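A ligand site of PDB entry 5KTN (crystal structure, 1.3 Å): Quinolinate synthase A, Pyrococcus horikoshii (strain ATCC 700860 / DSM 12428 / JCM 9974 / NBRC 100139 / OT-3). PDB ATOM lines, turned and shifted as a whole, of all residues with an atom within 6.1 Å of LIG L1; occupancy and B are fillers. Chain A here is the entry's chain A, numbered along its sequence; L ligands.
The side-chain carboxylate (OE1) of Glu 202 sits close to a sulfur (S2) of LIG L1, 3.5 Å away. Residues that only touch LIG L1: Tyr 27 (3.8 Å), Ala 88 (3.9 Å), Met 89 (3.6 Å), Tyr 175 (3.8 Å) and Val 176 (3.8 Å). Ten residues have an atom within 4 Å of LIG L1: Tyr 27, Cys 87, Ala 88, Met 89, Asn 115, Cys 174, Tyr 175, Val 176, Glu 202 and Cys 260. The nearest printed residue that does not touch LIG L1 is Val 62 (4.1 Å).
A sulfur (S2) of LIG L1 sits close to the side-chain amide nitrogen (ND2) of Asn 115 (3.4 Å). The side-chain sulfur (SG) of Cys 260 is bound to an iron atom (FE2) of LIG L1. SG of Cys 87 binds FE1 of LIG L1. SG of Cys 174 binds FE3 of LIG L1 (2.3 Å). An oxygen (O6) of LG2 L2 lies close to the side-chain carboxylate of Glu 202.
N of Ala 90 sits close to SG of Cys 87, at 3.4 Å. N of Cys 260 lies within hydrogen-bond range of OE2 of Glu 235 (2.8 Å). The backbone NH of Gly 262 sits close to the side-chain sulfur of Cys 260 (3.7 Å). The side-chain carboxylate (OE1) of Glu 202 lies within hydrogen-bond range of a ring nitrogen (ND1) of His 177 (3.1 Å). OH of Tyr 175 sits at hydrogen-bond distance from N of Ile 261. The side-chain sulfur of Cys 87 sits close to the side-chain amide nitrogen of Asn 115 (3.7 Å). The backbone NH of Val 176 sits close to the side-chain sulfur of Cys 174 (3.3 Å). The backbone NH (N) of Met 89 lies close to the side-chain sulfur (SG) of Cys 87, at 3.6 Å.
FE4 of LIG L1 is bound by O6 of LG2 L2 (2.2 Å).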
ATOM      1  N   TYR A  27      -6.957 -11.284  -7.280  1.00  0.00           N
ATOM      2  CA  TYR A  27      -5.850 -11.473  -6.351  1.00  0.00           C
ATOM      3  C   TYR A  27      -4.505 -11.073  -6.957  1.00  0.00           C
ATOM      4  O   TYR A  27      -3.463 -11.273  -6.315  1.00  0.00           O
ATOM      5  CB  TYR A  27      -5.746 -12.933  -5.893  1.00  0.00           C
ATOM      6  CG  TYR A  27      -6.939 -13.503  -5.148  1.00  0.00           C
ATOM      7  CD1 TYR A  27      -7.909 -12.685  -4.578  1.00  0.00           C
ATOM      8  CD2 TYR A  27      -7.081 -14.882  -5.010  1.00  0.00           C
ATOM      9  CE1 TYR A  27      -8.998 -13.230  -3.892  1.00  0.00           C
ATOM     10  CE2 TYR A  27      -8.147 -15.438  -4.335  1.00  0.00           C
ATOM     11  CZ  TYR A  27      -9.108 -14.620  -3.784  1.00  0.00           C
ATOM     12  OH  TYR A  27     -10.171 -15.220  -3.131  1.00  0.00           O
ATOM     13  N   VAL A  62      -4.011 -17.959 -12.260  1.00  0.00           N
ATOM     14  CA  VAL A  62      -3.443 -19.286 -12.108  1.00  0.00           C
ATOM     15  C   VAL A  62      -3.831 -20.231 -13.244  1.00  0.00           C
ATOM     16  O   VAL A  62      -4.740 -19.942 -14.042  1.00  0.00           O
ATOM     17  CB  VAL A  62      -3.777 -19.897 -10.731  1.00  0.00           C
ATOM     18  CG1 VAL A  62      -3.135 -19.063  -9.650  1.00  0.00           C
ATOM     19  CG2 VAL A  62      -5.293 -20.003 -10.561  1.00  0.00           C
ATOM     20  N   PHE A  64      -5.516 -23.046 -13.734  1.00  0.00           N
ATOM     21  CA  PHE A  64      -6.859 -23.522 -14.063  1.00  0.00           C
ATOM     22  C   PHE A  64      -7.682 -22.426 -14.732  1.00  0.00           C
ATOM     23  O   PHE A  64      -8.559 -22.721 -15.554  1.00  0.00           O
ATOM     24  CB  PHE A  64      -7.571 -24.153 -12.848  1.00  0.00           C
ATOM     25  CG  PHE A  64      -8.108 -23.147 -11.831  1.00  0.00           C
ATOM     26  CD1 PHE A  64      -9.304 -22.465 -12.052  1.00  0.00           C
ATOM     27  CD2 PHE A  64      -7.427 -22.931 -10.648  1.00  0.00           C
ATOM     28  CE1 PHE A  64      -9.786 -21.578 -11.120  1.00  0.00           C
ATOM     29  CE2 PHE A  64      -7.908 -22.036  -9.705  1.00  0.00           C
ATOM     30  CZ  PHE A  64      -9.083 -21.351  -9.938  1.00  0.00           C
ATOM     31  N   MET A  65      -7.406 -21.166 -14.404  1.00  0.00           N
ATOM     32  CA  MET A  65      -8.117 -20.059 -15.029  1.00  0.00           C
ATOM     33  C   MET A  65      -7.668 -19.872 -16.478  1.00  0.00           C
ATOM     34  O   MET A  65      -8.512 -19.694 -17.368  1.00  0.00           O
ATOM     35  CB  MET A  65      -7.893 -18.785 -14.226  1.00  0.00           C
ATOM     36  CG  MET A  65      -8.403 -18.889 -12.796  1.00  0.00           C
ATOM     37  SD  MET A  65      -8.075 -17.372 -11.883  1.00  0.00           S
ATOM     38  CE  MET A  65      -8.817 -17.807 -10.303  1.00  0.00           C
ATOM     39  N   THR A  86       0.007 -21.599 -10.033  1.00  0.00           N
ATOM     40  CA  THR A  86      -0.814 -22.795  -9.892  1.00  0.00           C
ATOM     41  C   THR A  86      -1.650 -22.705  -8.630  1.00  0.00           C
ATOM     42  O   THR A  86      -1.336 -21.982  -7.688  1.00  0.00           O
ATOM     43  CB  THR A  86       0.031 -24.082  -9.849  1.00  0.00           C
ATOM     44  OG1 THR A  86       0.981 -23.991  -8.782  1.00  0.00           O
ATOM     45  CG2 THR A  86       0.768 -24.312 -11.172  1.00  0.00           C
ATOM     46  N   CYS A  87      -2.758 -23.450  -8.646  1.00  0.00           N
ATOM     47  CA  CYS A  87      -3.676 -23.522  -7.516  1.00  0.00           C
ATOM     48  C   CYS A  87      -3.496 -24.849  -6.786  1.00  0.00           C
ATOM     49  O   CYS A  87      -3.774 -25.917  -7.357  1.00  0.00           O
ATOM     50  CB  CYS A  87      -5.123 -23.398  -7.989  1.00  0.00           C
ATOM     51  SG  CYS A  87      -6.345 -23.647  -6.697  1.00  0.00           S
ATOM     52  N   ALA A  88      -3.078 -24.773  -5.522  1.00  0.00           N
ATOM     53  CA  ALA A  88      -2.824 -25.979  -4.743  1.00  0.00           C
ATOM     54  C   ALA A  88      -4.087 -26.815  -4.592  1.00  0.00           C
ATOM     55  O   ALA A  88      -4.040 -28.050  -4.661  1.00  0.00           O
ATOM     56  CB  ALA A  88      -2.278 -25.605  -3.358  1.00  0.00           C
ATOM     57  N   MET A  89      -5.239 -26.152  -4.391  1.00  0.00           N
ATOM     58  CA  MET A  89      -6.498 -26.841  -4.169  1.00  0.00           C
ATOM     59  C   MET A  89      -6.960 -27.588  -5.417  1.00  0.00           C
ATOM     60  O   MET A  89      -7.456 -28.720  -5.328  1.00  0.00           O
ATOM     61  CB  MET A  89      -7.568 -25.830  -3.724  1.00  0.00           C
ATOM     62  CG  MET A  89      -8.950 -26.445  -3.406  1.00  0.00           C
ATOM     63  SD  MET A  89     -10.202 -26.103  -4.660  1.00  0.00           S
ATOM     64  CE  MET A  89     -10.441 -24.361  -4.391  1.00  0.00           C
ATOM     65  N   ALA A  90      -6.801 -26.969  -6.590  1.00  0.00           N
ATOM     66  CA  ALA A  90      -7.229 -27.575  -7.843  1.00  0.00           C
ATOM     67  C   ALA A  90      -6.480 -28.872  -8.103  1.00  0.00           C
ATOM     68  O   ALA A  90      -7.057 -29.856  -8.597  1.00  0.00           O
ATOM     69  CB  ALA A  90      -6.982 -26.591  -8.980  1.00  0.00           C
ATOM     70  N   TYR A 113     -15.777 -27.738  -9.112  1.00  0.00           N
ATOM     71  CA  TYR A 113     -15.293 -26.373  -8.983  1.00  0.00           C
ATOM     72  C   TYR A 113     -14.396 -26.071 -10.166  1.00  0.00           C
ATOM     73  O   TYR A 113     -13.638 -26.935 -10.628  1.00  0.00           O
ATOM     74  CB  TYR A 113     -14.465 -26.287  -7.697  1.00  0.00           C
ATOM     75  CG  TYR A 113     -14.426 -24.966  -6.972  1.00  0.00           C
ATOM     76  CD1 TYR A 113     -15.217 -23.877  -7.347  1.00  0.00           C
ATOM     77  CD2 TYR A 113     -13.593 -24.805  -5.883  1.00  0.00           C
ATOM     78  CE1 TYR A 113     -15.155 -22.683  -6.657  1.00  0.00           C
ATOM     79  CE2 TYR A 113     -13.520 -23.617  -5.199  1.00  0.00           C
ATOM     80  CZ  TYR A 113     -14.300 -22.570  -5.581  1.00  0.00           C
ATOM     81  OH  TYR A 113     -14.201 -21.398  -4.862  1.00  0.00           O
ATOM     82  N   ASN A 115     -11.766 -24.521 -10.007  1.00  0.00           N
ATOM     83  CA  ASN A 115     -10.449 -24.889  -9.478  1.00  0.00           C
ATOM     84  C   ASN A 115     -10.272 -26.398  -9.653  1.00  0.00           C
ATOM     85  O   ASN A 115     -10.449 -27.176  -8.713  1.00  0.00           O
ATOM     86  CB  ASN A 115     -10.321 -24.534  -7.997  1.00  0.00           C
ATOM     87  CG  ASN A 115     -10.693 -23.088  -7.695  1.00  0.00           C
ATOM     88  OD1 ASN A 115     -11.752 -22.597  -8.097  1.00  0.00           O
ATOM     89  ND2 ASN A 115      -9.813 -22.405  -6.967  1.00  0.00           N
ATOM     90  N   ASP A 150     -13.261 -28.413  -3.178  1.00  0.00           N
ATOM     91  CA  ASP A 150     -13.177 -27.655  -1.926  1.00  0.00           C
ATOM     92  C   ASP A 150     -14.260 -28.102  -0.947  1.00  0.00           C
ATOM     93  O   ASP A 150     -15.448 -27.892  -1.181  1.00  0.00           O
ATOM     94  CB  ASP A 150     -13.269 -26.153  -2.199  1.00  0.00           C
ATOM     95  CG  ASP A 150     -12.889 -25.335  -1.002  1.00  0.00           C
ATOM     96  OD1 ASP A 150     -11.785 -24.747  -0.988  1.00  0.00           O
ATOM     97  OD2 ASP A 150     -13.691 -25.292  -0.035  1.00  0.00           O
ATOM     98  N   CYS A 174      -8.322 -24.837   0.416  1.00  0.00           N
ATOM     99  CA  CYS A 174      -7.397 -23.790   0.035  1.00  0.00           C
ATOM    100  C   CYS A 174      -6.599 -23.340   1.255  1.00  0.00           C
ATOM    101  O   CYS A 174      -7.188 -22.845   2.230  1.00  0.00           O
ATOM    102  CB  CYS A 174      -8.180 -22.596  -0.524  1.00  0.00           C
ATOM    103  SG  CYS A 174      -7.176 -21.087  -0.661  1.00  0.00           S
ATOM    104  N   TYR A 175      -5.271 -23.497   1.202  1.00  0.00           N
ATOM    105  CA  TYR A 175      -4.439 -23.111   2.359  1.00  0.00           C
ATOM    106  C   TYR A 175      -4.562 -21.622   2.673  1.00  0.00           C
ATOM    107  O   TYR A 175      -4.390 -21.228   3.841  1.00  0.00           O
ATOM    108  CB  TYR A 175      -2.967 -23.493   2.141  1.00  0.00           C
ATOM    109  CG  TYR A 175      -2.261 -22.682   1.070  1.00  0.00           C
ATOM    110  CD1 TYR A 175      -1.524 -21.549   1.399  1.00  0.00           C
ATOM    111  CD2 TYR A 175      -2.360 -23.040  -0.274  1.00  0.00           C
ATOM    112  CE1 TYR A 175      -0.872 -20.806   0.413  1.00  0.00           C
ATOM    113  CE2 TYR A 175      -1.727 -22.284  -1.258  1.00  0.00           C
ATOM    114  CZ  TYR A 175      -0.984 -21.163  -0.904  1.00  0.00           C
ATOM    115  OH  TYR A 175      -0.347 -20.406  -1.864  1.00  0.00           O
ATOM    116  N   VAL A 176      -4.811 -20.778   1.669  1.00  0.00           N
ATOM    117  CA  VAL A 176      -4.924 -19.349   1.920  1.00  0.00           C
ATOM    118  C   VAL A 176      -6.098 -19.056   2.829  1.00  0.00           C
ATOM    119  O   VAL A 176      -5.974 -18.370   3.844  1.00  0.00           O
ATOM    120  CB  VAL A 176      -5.047 -18.579   0.588  1.00  0.00           C
ATOM    121  CG1 VAL A 176      -5.114 -17.063   0.861  1.00  0.00           C
ATOM    122  CG2 VAL A 176      -3.887 -18.926  -0.352  1.00  0.00           C
ATOM    123  N   HIS A 177      -7.270 -19.552   2.450  1.00  0.00           N
ATOM    124  CA  HIS A 177      -8.475 -19.293   3.221  1.00  0.00           C
ATOM    125  C   HIS A 177      -8.510 -20.043   4.543  1.00  0.00           C
ATOM    126  O   HIS A 177      -9.178 -19.590   5.468  1.00  0.00           O
ATOM    127  CB  HIS A 177      -9.718 -19.534   2.365  1.00  0.00           C
ATOM    128  CG  HIS A 177      -9.891 -18.498   1.301  1.00  0.00           C
ATOM    129  ND1 HIS A 177      -9.346 -18.623   0.041  1.00  0.00           N
ATOM    130  CD2 HIS A 177     -10.497 -17.280   1.330  1.00  0.00           C
ATOM    131  CE1 HIS A 177      -9.630 -17.545  -0.665  1.00  0.00           C
ATOM    132  NE2 HIS A 177     -10.322 -16.713   0.097  1.00  0.00           N
ATOM    133  N   GLU A 202     -14.575 -20.379   0.734  1.00  0.00           N
ATOM    134  CA  GLU A 202     -13.435 -21.263   0.960  1.00  0.00           C
ATOM    135  C   GLU A 202     -12.933 -21.200   2.398  1.00  0.00           C
ATOM    136  O   GLU A 202     -12.093 -22.024   2.777  1.00  0.00           O
ATOM    137  CB  GLU A 202     -12.318 -20.976  -0.049  1.00  0.00           C
ATOM    138  CG  GLU A 202     -12.691 -21.385  -1.483  1.00  0.00           C
ATOM    139  CD  GLU A 202     -11.709 -20.877  -2.523  1.00  0.00           C
ATOM    140  OE1 GLU A 202     -10.639 -20.386  -2.115  1.00  0.00           O
ATOM    141  OE2 GLU A 202     -12.006 -20.962  -3.738  1.00  0.00           O
ATOM    142  N   GLU A 235      -8.055 -13.461   0.141  1.00  0.00           N
ATOM    143  CA  GLU A 235      -6.672 -13.168  -0.180  1.00  0.00           C
ATOM    144  C   GLU A 235      -6.468 -11.659  -0.197  1.00  0.00           C
ATOM    145  O   GLU A 235      -7.291 -10.912  -0.714  1.00  0.00           O
ATOM    146  CB  GLU A 235      -6.356 -13.761  -1.558  1.00  0.00           C
ATOM    147  CG  GLU A 235      -4.914 -14.184  -1.781  1.00  0.00           C
ATOM    148  CD  GLU A 235      -4.007 -13.061  -2.282  1.00  0.00           C
ATOM    149  OE1 GLU A 235      -4.489 -11.919  -2.494  1.00  0.00           O
ATOM    150  OE2 GLU A 235      -2.798 -13.323  -2.494  1.00  0.00           O
ATOM    151  N   CYS A 260      -1.784 -15.856  -1.792  1.00  0.00           N
ATOM    152  CA  CYS A 260      -1.754 -17.000  -2.704  1.00  0.00           C
ATOM    153  C   CYS A 260      -0.430 -16.964  -3.480  1.00  0.00           C
ATOM    154  O   CYS A 260      -0.238 -16.099  -4.334  1.00  0.00           O
ATOM    155  CB  CYS A 260      -2.935 -16.960  -3.671  1.00  0.00           C
ATOM    156  SG  CYS A 260      -2.884 -18.318  -4.875  1.00  0.00           S
ATOM    157  N   ILE A 261       0.441 -17.933  -3.210  1.00  0.00           N
ATOM    158  CA  ILE A 261       1.742 -17.972  -3.865  1.00  0.00           C
ATOM    159  C   ILE A 261       1.579 -18.097  -5.371  1.00  0.00           C
ATOM    160  O   ILE A 261       2.304 -17.460  -6.145  1.00  0.00           O
ATOM    161  CB  ILE A 261       2.571 -19.129  -3.283  1.00  0.00           C
ATOM    162  CG1 ILE A 261       2.934 -18.834  -1.821  1.00  0.00           C
ATOM    163  CG2 ILE A 261       3.819 -19.415  -4.133  1.00  0.00           C
ATOM    164  CD1 ILE A 261       3.426 -20.021  -1.048  1.00  0.00           C
ATOM    165  N   GLY A 262       0.626 -18.911  -5.825  1.00  0.00           N
ATOM    166  CA  GLY A 262       0.436 -19.093  -7.256  1.00  0.00           C
ATOM    167  C   GLY A 262       0.047 -17.809  -7.966  1.00  0.00           C
ATOM    168  O   GLY A 262       0.581 -17.481  -9.037  1.00  0.00           O
ATOM    169  N   MET A 263      -0.901 -17.059  -7.386  1.00  0.00           N
ATOM    170  CA  MET A 263      -1.290 -15.782  -7.964  1.00  0.00           C
ATOM    171  C   MET A 263      -0.088 -14.852  -8.088  1.00  0.00           C
ATOM    172  O   MET A 263       0.076 -14.173  -9.114  1.00  0.00           O
ATOM    173  CB  MET A 263      -2.373 -15.135  -7.106  1.00  0.00           C
ATOM    174  CG  MET A 263      -3.721 -15.801  -7.261  1.00  0.00           C
ATOM    175  SD  MET A 263      -4.456 -15.450  -8.887  1.00  0.00           S
ATOM    176  CE  MET A 263      -6.004 -16.371  -8.742  1.00  0.00           C
HETATM  177 FE1  LIG L   1      -6.183 -21.757  -5.349  1.00  0.00          FE
HETATM  178 FE2  LIG L   1      -4.839 -19.513  -4.633  1.00  0.00          FE
HETATM  179 FE3  LIG L   1      -6.475 -20.794  -2.854  1.00  0.00          FE
HETATM  180 FE4  LIG L   1      -7.713 -19.522  -4.882  1.00  0.00          FE
HETATM  181  S1  LIG L   1      -6.328 -18.556  -3.235  1.00  0.00           S
HETATM  182  S2  LIG L   1      -8.106 -21.661  -4.163  1.00  0.00           S
HETATM  183  S3  LIG L   1      -6.022 -19.871  -6.530  1.00  0.00           S
HETATM  184  S4  LIG L   1      -4.538 -21.643  -3.741  1.00  0.00           S
HETATM  185  P1  LG2 L   2     -13.426 -16.315  -6.830  1.00  0.00           P
HETATM  186  O1  LG2 L   2     -12.610 -15.162  -7.320  1.00  0.00           O
HETATM  187  O2  LG2 L   2     -14.265 -16.996  -7.984  1.00  0.00           O
HETATM  188  O3  LG2 L   2     -14.353 -15.904  -5.609  1.00  0.00           O
HETATM  189  O4  LG2 L   2     -12.470 -17.437  -6.196  1.00  0.00           O
HETATM  190  C1  LG2 L   2     -11.325 -17.713  -6.986  1.00  0.00           C
HETATM  191  C2  LG2 L   2     -10.303 -18.321  -6.047  1.00  0.00           C
HETATM  192  O5  LG2 L   2      -9.126 -18.691  -6.544  1.00  0.00           O
HETATM  193  C3  LG2 L   2     -10.480 -18.212  -4.607  1.00  0.00           C
HETATM  194  O6  LG2 L   2      -9.510 -18.788  -3.849  1.00  0.00           O
